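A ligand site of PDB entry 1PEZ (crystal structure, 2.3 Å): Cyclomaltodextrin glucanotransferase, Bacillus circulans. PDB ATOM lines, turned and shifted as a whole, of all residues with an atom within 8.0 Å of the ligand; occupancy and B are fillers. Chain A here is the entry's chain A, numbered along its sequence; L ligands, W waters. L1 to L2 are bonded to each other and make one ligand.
The backbone carbonyl oxygen of Thr 598 is in hydrogen-bond range of an oxygen (O2) of LIG L1 (2.6 Å). An oxygen (O1) of LG2 L2 sits at hydrogen-bond distance from the backbone carbonyl oxygen of Gln 602 (2.7 Å). The side-chain hydroxyl of Thr 598 sits at hydrogen-bond distance from an oxygen (O3) of LIG L1. The backbone NH (N) of Gly 601 lies within hydrogen-bond range of an oxygen (O2) of LG2 L2, 3.1 Å away. The side-chain amide nitrogen (NE2) of Gln 628 is in hydrogen-bond range of an oxygen (O5) of LG2 L2 (2.9 Å). O5 of LG2 L2 lies within hydrogen-bond range of OD1 of Asn 627 (2.7 Å). The backbone carbonyl oxygen of Ala 599 sits at hydrogen-bond distance from an oxygen (O1) of LG2 L2, 3.2 Å away.
The side-chain hydroxyl of Tyr 633 sits at hydrogen-bond distance from the backbone NH of Thr 598, 2.7 Å away. The backbone carbonyl oxygen (O) of Asn 627 lies within hydrogen-bond range of the backbone NH (N) of Tyr 633. The backbone NH (N) of Gln 628 is in hydrogen-bond range of the side-chain carboxylate (OE2) of Glu 187 (2.7 Å). NE1 of Trp 636 sits close to O of Pro 634 (3.5 Å). The side-chain amide oxygen of Gln 628 lies within hydrogen-bond range of the side-chain hydroxyl of Thr 185, 3.1 Å away. The side-chain amide oxygen (OE1) of Gln 602 sits at hydrogen-bond distance from the backbone NH (N) of Ala 599, 3.0 Å away. The side-chain amide nitrogen of Gln 632 sits at hydrogen-bond distance from the backbone carbonyl oxygen of Gln 628, at 3.1 Å. The indole nitrogen (NE1) of Trp 636 lies within hydrogen-bond range of the backbone carbonyl oxygen (O) of Ala 596.
N of Leu 600 touches O3 of LIG L1, 3.5 Å away. OD1 of Asn 603 touches C2 of LG2 L2, 3.2 Å away. CZ of Tyr 633 touches C2 of LIG L1, at 3.6 Å. Trp 636 touches the ligand. Hydrophobic or aromatic side chains that line the ligand: Tyr 633 and Trp 636.
Water W1 lies within hydrogen-bond range of ND2 of Asn 603 and O2 of LG2 L2. Water W2 lies within hydrogen-bond range of O of Asn 627 (2.9 Å) and O6 of LIG L1 (3.4 Å).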
ATOM      1  N   THR A 185      13.454 -18.670 -10.907  1.00  0.00           N
ATOM      2  CA  THR A 185      13.332 -19.063  -9.496  1.00  0.00           C
ATOM      3  C   THR A 185      12.363 -18.113  -8.823  1.00  0.00           C
ATOM      4  O   THR A 185      12.160 -16.988  -9.287  1.00  0.00           O
ATOM      5  CB  THR A 185      14.682 -18.997  -8.745  1.00  0.00           C
ATOM      6  OG1 THR A 185      15.064 -17.631  -8.556  1.00  0.00           O
ATOM      7  CG2 THR A 185      15.778 -19.734  -9.510  1.00  0.00           C
ATOM      8  N   GLU A 187      12.721 -16.477  -6.071  1.00  0.00           N
ATOM      9  CA  GLU A 187      13.469 -15.291  -5.656  1.00  0.00           C
ATOM     10  C   GLU A 187      13.664 -14.326  -6.821  1.00  0.00           C
ATOM     11  O   GLU A 187      13.526 -13.114  -6.669  1.00  0.00           O
ATOM     12  CB  GLU A 187      14.845 -15.697  -5.111  1.00  0.00           C
ATOM     13  CG  GLU A 187      15.666 -14.518  -4.603  1.00  0.00           C
ATOM     14  CD  GLU A 187      17.082 -14.906  -4.233  1.00  0.00           C
ATOM     15  OE1 GLU A 187      17.358 -16.115  -4.043  1.00  0.00           O
ATOM     16  OE2 GLU A 187      17.923 -14.003  -4.118  1.00  0.00           O
ATOM     17  N   ALA A 596      27.361 -17.515   5.493  1.00  0.00           N
ATOM     18  CA  ALA A 596      26.678 -18.734   5.866  1.00  0.00           C
ATOM     19  C   ALA A 596      26.865 -19.750   4.735  1.00  0.00           C
ATOM     20  O   ALA A 596      26.017 -19.866   3.839  1.00  0.00           O
ATOM     21  CB  ALA A 596      25.189 -18.459   6.088  1.00  0.00           C
ATOM     22  N   THR A 597      27.986 -20.464   4.779  1.00  0.00           N
ATOM     23  CA  THR A 597      28.296 -21.463   3.753  1.00  0.00           C
ATOM     24  C   THR A 597      27.485 -22.745   3.919  1.00  0.00           C
ATOM     25  O   THR A 597      27.206 -23.189   5.028  1.00  0.00           O
ATOM     26  CB  THR A 597      29.800 -21.833   3.761  1.00  0.00           C
ATOM     27  OG1 THR A 597      30.182 -22.273   5.073  1.00  0.00           O
ATOM     28  CG2 THR A 597      30.644 -20.633   3.352  1.00  0.00           C
ATOM     29  N   THR A 598      27.119 -23.328   2.789  1.00  0.00           N
ATOM     30  CA  THR A 598      26.298 -24.535   2.775  1.00  0.00           C
ATOM     31  C   THR A 598      26.727 -25.481   1.652  1.00  0.00           C
ATOM     32  O   THR A 598      27.479 -25.104   0.753  1.00  0.00           O
ATOM     33  CB  THR A 598      24.817 -24.188   2.534  1.00  0.00           C
ATOM     34  OG1 THR A 598      24.710 -23.403   1.343  1.00  0.00           O
ATOM     35  CG2 THR A 598      24.257 -23.396   3.709  1.00  0.00           C
ATOM     36  N   ALA A 599      26.230 -26.705   1.722  1.00  0.00           N
ATOM     37  CA  ALA A 599      26.477 -27.703   0.691  1.00  0.00           C
ATOM     38  C   ALA A 599      25.196 -27.743  -0.132  1.00  0.00           C
ATOM     39  O   ALA A 599      24.128 -27.377   0.373  1.00  0.00           O
ATOM     40  CB  ALA A 599      26.741 -29.069   1.314  1.00  0.00           C
ATOM     41  N   LEU A 600      25.286 -28.174  -1.385  1.00  0.00           N
ATOM     42  CA  LEU A 600      24.109 -28.239  -2.243  1.00  0.00           C
ATOM     43  C   LEU A 600      22.959 -28.989  -1.587  1.00  0.00           C
ATOM     44  O   LEU A 600      23.128 -30.091  -1.069  1.00  0.00           O
ATOM     45  CB  LEU A 600      24.467 -28.899  -3.578  1.00  0.00           C
ATOM     46  CG  LEU A 600      25.013 -27.948  -4.647  1.00  0.00           C
ATOM     47  CD1 LEU A 600      25.445 -28.726  -5.877  1.00  0.00           C
ATOM     48  CD2 LEU A 600      23.931 -26.923  -5.007  1.00  0.00           C
ATOM     49  N   GLY A 601      21.775 -28.380  -1.616  1.00  0.00           N
ATOM     50  CA  GLY A 601      20.604 -28.992  -1.015  1.00  0.00           C
ATOM     51  C   GLY A 601      20.370 -28.486   0.393  1.00  0.00           C
ATOM     52  O   GLY A 601      19.280 -28.633   0.952  1.00  0.00           O
ATOM     53  N   GLN A 602      21.410 -27.900   0.965  1.00  0.00           N
ATOM     54  CA  GLN A 602      21.367 -27.351   2.324  1.00  0.00           C
ATOM     55  C   GLN A 602      21.090 -25.852   2.246  1.00  0.00           C
ATOM     56  O   GLN A 602      21.728 -25.135   1.477  1.00  0.00           O
ATOM     57  CB  GLN A 602      22.701 -27.616   3.014  1.00  0.00           C
ATOM     58  CG  GLN A 602      22.817 -27.056   4.425  1.00  0.00           C
ATOM     59  CD  GLN A 602      24.147 -27.417   5.069  1.00  0.00           C
ATOM     60  OE1 GLN A 602      25.212 -27.152   4.516  1.00  0.00           O
ATOM     61  NE2 GLN A 602      24.092 -28.036   6.248  1.00  0.00           N
ATOM     62  N   ASN A 603      20.130 -25.373   3.032  1.00  0.00           N
ATOM     63  CA  ASN A 603      19.757 -23.961   3.014  1.00  0.00           C
ATOM     64  C   ASN A 603      19.716 -23.339   4.409  1.00  0.00           C
ATOM     65  O   ASN A 603      19.606 -24.042   5.412  1.00  0.00           O
ATOM     66  CB  ASN A 603      18.396 -23.794   2.349  1.00  0.00           C
ATOM     67  CG  ASN A 603      18.426 -24.137   0.869  1.00  0.00           C
ATOM     68  OD1 ASN A 603      18.920 -23.358   0.049  1.00  0.00           O
ATOM     69  ND2 ASN A 603      17.893 -25.294   0.523  1.00  0.00           N
ATOM     70  N   VAL A 604      19.805 -22.020   4.450  1.00  0.00           N
ATOM     71  CA  VAL A 604      19.770 -21.299   5.723  1.00  0.00           C
ATOM     72  C   VAL A 604      18.347 -20.856   6.056  1.00  0.00           C
ATOM     73  O   VAL A 604      17.603 -20.414   5.179  1.00  0.00           O
ATOM     74  CB  VAL A 604      20.688 -20.057   5.686  1.00  0.00           C
ATOM     75  CG1 VAL A 604      20.611 -19.317   7.016  1.00  0.00           C
ATOM     76  CG2 VAL A 604      22.115 -20.484   5.391  1.00  0.00           C
ATOM     77  N   PRO A 624      13.270 -21.711   3.180  1.00  0.00           N
ATOM     78  CA  PRO A 624      14.676 -21.290   3.017  1.00  0.00           C
ATOM     79  C   PRO A 624      14.843 -19.825   2.613  1.00  0.00           C
ATOM     80  O   PRO A 624      14.024 -19.262   1.891  1.00  0.00           O
ATOM     81  CB  PRO A 624      15.202 -22.254   1.962  1.00  0.00           C
ATOM     82  CG  PRO A 624      13.971 -22.620   1.174  1.00  0.00           C
ATOM     83  CD  PRO A 624      12.946 -22.802   2.260  1.00  0.00           C
ATOM     84  N   MET A 625      15.926 -19.214   3.102  1.00  0.00           N
ATOM     85  CA  MET A 625      16.221 -17.819   2.800  1.00  0.00           C
ATOM     86  C   MET A 625      16.784 -17.687   1.388  1.00  0.00           C
ATOM     87  O   MET A 625      17.104 -18.690   0.747  1.00  0.00           O
ATOM     88  CB  MET A 625      17.201 -17.264   3.828  1.00  0.00           C
ATOM     89  CG  MET A 625      16.614 -17.203   5.245  1.00  0.00           C
ATOM     90  SD  MET A 625      17.763 -16.636   6.505  1.00  0.00           S
ATOM     91  CE  MET A 625      17.973 -14.909   6.031  1.00  0.00           C
ATOM     92  N   TYR A 626      16.916 -16.453   0.915  1.00  0.00           N
ATOM     93  CA  TYR A 626      17.432 -16.192  -0.427  1.00  0.00           C
ATOM     94  C   TYR A 626      18.898 -15.793  -0.417  1.00  0.00           C
ATOM     95  O   TYR A 626      19.425 -15.329   0.600  1.00  0.00           O
ATOM     96  CB  TYR A 626      16.604 -15.102  -1.119  1.00  0.00           C
ATOM     97  CG  TYR A 626      15.136 -15.441  -1.276  1.00  0.00           C
ATOM     98  CD1 TYR A 626      14.725 -16.725  -1.614  1.00  0.00           C
ATOM     99  CD2 TYR A 626      14.148 -14.459  -1.112  1.00  0.00           C
ATOM    100  CE1 TYR A 626      13.378 -17.033  -1.793  1.00  0.00           C
ATOM    101  CE2 TYR A 626      12.803 -14.750  -1.291  1.00  0.00           C
ATOM    102  CZ  TYR A 626      12.420 -16.038  -1.624  1.00  0.00           C
ATOM    103  OH  TYR A 626      11.089 -16.330  -1.801  1.00  0.00           O
ATOM    104  N   ASN A 627      19.562 -15.981  -1.555  1.00  0.00           N
ATOM    105  CA  ASN A 627      20.982 -15.657  -1.679  1.00  0.00           C
ATOM    106  C   ASN A 627      21.376 -15.397  -3.126  1.00  0.00           C
ATOM    107  O   ASN A 627      22.495 -15.696  -3.538  1.00  0.00           O
ATOM    108  CB  ASN A 627      21.837 -16.800  -1.117  1.00  0.00           C
ATOM    109  CG  ASN A 627      21.600 -18.114  -1.840  1.00  0.00           C
ATOM    110  OD1 ASN A 627      21.096 -18.138  -2.970  1.00  0.00           O
ATOM    111  ND2 ASN A 627      21.969 -19.217  -1.210  1.00  0.00           N
ATOM    112  N   GLN A 628      20.459 -14.827  -3.907  1.00  0.00           N
ATOM    113  CA  GLN A 628      20.712 -14.562  -5.320  1.00  0.00           C
ATOM    114  C   GLN A 628      20.664 -13.089  -5.722  1.00  0.00           C
ATOM    115  O   GLN A 628      21.671 -12.518  -6.155  1.00  0.00           O
ATOM    116  CB  GLN A 628      19.702 -15.327  -6.180  1.00  0.00           C
ATOM    117  CG  GLN A 628      19.968 -16.830  -6.326  1.00  0.00           C
ATOM    118  CD  GLN A 628      18.756 -17.594  -6.869  1.00  0.00           C
ATOM    119  OE1 GLN A 628      17.888 -17.024  -7.540  1.00  0.00           O
ATOM    120  NE2 GLN A 628      18.709 -18.883  -6.580  1.00  0.00           N
ATOM    121  N   VAL A 629      19.497 -12.486  -5.568  1.00  0.00           N
ATOM    122  CA  VAL A 629      19.265 -11.110  -6.004  1.00  0.00           C
ATOM    123  C   VAL A 629      19.784  -9.976  -5.121  1.00  0.00           C
ATOM    124  O   VAL A 629      20.821  -9.369  -5.432  1.00  0.00           O
ATOM    125  CB  VAL A 629      17.756 -10.880  -6.291  1.00  0.00           C
ATOM    126  CG1 VAL A 629      17.530  -9.492  -6.867  1.00  0.00           C
ATOM    127  CG2 VAL A 629      17.245 -11.947  -7.241  1.00  0.00           C
ATOM    128  N   GLN A 632      24.169 -11.946  -2.330  1.00  0.00           N
ATOM    129  CA  GLN A 632      24.676 -13.158  -2.965  1.00  0.00           C
ATOM    130  C   GLN A 632      25.354 -14.084  -1.961  1.00  0.00           C
ATOM    131  O   GLN A 632      25.974 -13.638  -0.998  1.00  0.00           O
ATOM    132  CB  GLN A 632      25.670 -12.809  -4.078  1.00  0.00           C
ATOM    133  CG  GLN A 632      25.089 -11.972  -5.220  1.00  0.00           C
ATOM    134  CD  GLN A 632      24.690 -10.584  -4.772  1.00  0.00           C
ATOM    135  OE1 GLN A 632      25.500  -9.829  -4.230  1.00  0.00           O
ATOM    136  NE2 GLN A 632      23.433 -10.223  -5.017  1.00  0.00           N
ATOM    137  N   TYR A 633      25.245 -15.384  -2.206  1.00  0.00           N
ATOM    138  CA  TYR A 633      25.873 -16.389  -1.358  1.00  0.00           C
ATOM    139  C   TYR A 633      27.353 -16.016  -1.210  1.00  0.00           C
ATOM    140  O   TYR A 633      27.959 -15.491  -2.145  1.00  0.00           O
ATOM    141  CB  TYR A 633      25.712 -17.766  -2.010  1.00  0.00           C
ATOM    142  CG  TYR A 633      26.418 -18.882  -1.287  1.00  0.00           C
ATOM    143  CD1 TYR A 633      27.760 -19.176  -1.544  1.00  0.00           C
ATOM    144  CD2 TYR A 633      25.749 -19.641  -0.327  1.00  0.00           C
ATOM    145  CE1 TYR A 633      28.408 -20.203  -0.858  1.00  0.00           C
ATOM    146  CE2 TYR A 633      26.391 -20.656   0.362  1.00  0.00           C
ATOM    147  CZ  TYR A 633      27.720 -20.937   0.097  1.00  0.00           C
ATOM    148  OH  TYR A 633      28.364 -21.935   0.787  1.00  0.00           O
ATOM    149  N   PRO A 634      27.965 -16.300  -0.052  1.00  0.00           N
ATOM    150  CA  PRO A 634      27.416 -16.945   1.153  1.00  0.00           C
ATOM    151  C   PRO A 634      26.547 -16.051   2.049  1.00  0.00           C
ATOM    152  O   PRO A 634      26.352 -16.360   3.221  1.00  0.00           O
ATOM    153  CB  PRO A 634      28.667 -17.431   1.871  1.00  0.00           C
ATOM    154  CG  PRO A 634      29.641 -16.331   1.584  1.00  0.00           C
ATOM    155  CD  PRO A 634      29.415 -16.065   0.110  1.00  0.00           C
ATOM    156  N   TRP A 636      22.861 -14.522   2.965  1.00  0.00           N
ATOM    157  CA  TRP A 636      21.468 -14.883   2.768  1.00  0.00           C
ATOM    158  C   TRP A 636      20.556 -13.809   3.331  1.00  0.00           C
ATOM    159  O   TRP A 636      20.917 -13.106   4.276  1.00  0.00           O
ATOM    160  CB  TRP A 636      21.153 -16.217   3.458  1.00  0.00           C
ATOM    161  CG  TRP A 636      22.024 -17.365   3.035  1.00  0.00           C
ATOM    162  CD1 TRP A 636      23.374 -17.488   3.242  1.00  0.00           C
ATOM    163  CD2 TRP A 636      21.613 -18.560   2.354  1.00  0.00           C
ATOM    164  NE1 TRP A 636      23.812 -18.696   2.741  1.00  0.00           N
ATOM    165  CE2 TRP A 636      22.752 -19.370   2.199  1.00  0.00           C
ATOM    166  CE3 TRP A 636      20.378 -19.030   1.871  1.00  0.00           C
ATOM    167  CZ2 TRP A 636      22.708 -20.626   1.573  1.00  0.00           C
ATOM    168  CZ3 TRP A 636      20.327 -20.268   1.257  1.00  0.00           C
ATOM    169  CH2 TRP A 636      21.490 -21.051   1.110  1.00  0.00           C
ATOM    170  N   LYS A 655      19.738 -26.097   7.254  1.00  0.00           N
ATOM    171  CA  LYS A 655      18.932 -27.311   7.234  1.00  0.00           C
ATOM    172  C   LYS A 655      18.952 -28.082   5.932  1.00  0.00           C
ATOM    173  O   LYS A 655      18.996 -27.514   4.844  1.00  0.00           O
ATOM    174  CB  LYS A 655      17.471 -26.969   7.558  1.00  0.00           C
ATOM    175  CG  LYS A 655      17.211 -26.444   8.963  1.00  0.00           C
ATOM    176  CD  LYS A 655      15.732 -26.133   9.138  1.00  0.00           C
ATOM    177  CE  LYS A 655      14.879 -27.378   8.920  1.00  0.00           C
ATOM    178  NZ  LYS A 655      13.423 -27.057   8.888  1.00  0.00           N
ATOM    179  N   GLN A 656      18.896 -29.402   6.061  1.00  0.00           N
ATOM    180  CA  GLN A 656      18.791 -30.310   4.933  1.00  0.00           C
ATOM    181  C   GLN A 656      17.750 -31.299   5.417  1.00  0.00           C
ATOM    182  O   GLN A 656      17.994 -32.065   6.357  1.00  0.00           O
ATOM    183  CB  GLN A 656      20.125 -31.009   4.650  1.00  0.00           C
ATOM    184  CG  GLN A 656      20.107 -31.908   3.428  1.00  0.00           C
ATOM    185  CD  GLN A 656      21.474 -32.086   2.813  1.00  0.00           C
ATOM    186  OE1 GLN A 656      22.442 -32.422   3.496  1.00  0.00           O
ATOM    187  NE2 GLN A 656      21.566 -31.863   1.498  1.00  0.00           N
HETATM  188  C1  LIG L   1      27.485 -22.969  -3.452  1.00  0.00           C
HETATM  189  C2  LIG L   1      26.963 -23.625  -2.189  1.00  0.00           C
HETATM  190  C3  LIG L   1      25.523 -24.056  -2.403  1.00  0.00           C
HETATM  191  C4  LIG L   1      24.677 -22.826  -2.770  1.00  0.00           C
HETATM  192  C5  LIG L   1      25.231 -22.200  -4.071  1.00  0.00           C
HETATM  193  C6  LIG L   1      24.421 -20.961  -4.428  1.00  0.00           C
HETATM  194  O1  LIG L   1      27.589 -23.926  -4.461  1.00  0.00           O
HETATM  195  O2  LIG L   1      27.771 -24.747  -1.836  1.00  0.00           O
HETATM  196  O3  LIG L   1      25.051 -24.650  -1.201  1.00  0.00           O
HETATM  197  O4  LIG L   1      23.295 -23.203  -3.003  1.00  0.00           O
HETATM  198  O5  LIG L   1      26.614 -21.847  -3.810  1.00  0.00           O
HETATM  199  O6  LIG L   1      24.926 -20.377  -5.622  1.00  0.00           O
HETATM  200  C1  LG2 L   2      22.294 -22.845  -2.058  1.00  0.00           C
HETATM  201  C2  LG2 L   2      21.528 -24.123  -1.642  1.00  0.00           C
HETATM  202  C3  LG2 L   2      20.799 -24.697  -2.842  1.00  0.00           C
HETATM  203  C4  LG2 L   2      19.854 -23.634  -3.382  1.00  0.00           C
HETATM  204  C5  LG2 L   2      20.632 -22.364  -3.781  1.00  0.00           C
HETATM  205  C6  LG2 L   2      19.777 -21.288  -4.288  1.00  0.00           C
HETATM  206  O1  LG2 L   2      22.394 -25.131  -1.118  1.00  0.00           O
HETATM  207  O2  LG2 L   2      20.083 -25.878  -2.459  1.00  0.00           O
HETATM  208  O3  LG2 L   2      19.193 -24.093  -4.567  1.00  0.00           O
HETATM  209  O4  LG2 L   2      21.391 -21.848  -2.637  1.00  0.00           O
HETATM  210  O5  LG2 L   2      20.527 -20.116  -4.661  1.00  0.00           O
HETATM  211  O   HOH W   1      17.046 -26.212  -2.120  1.00  0.00           O
HETATM  212  O   HOH W   2      23.285 -17.455  -5.659  1.00  0.00           O
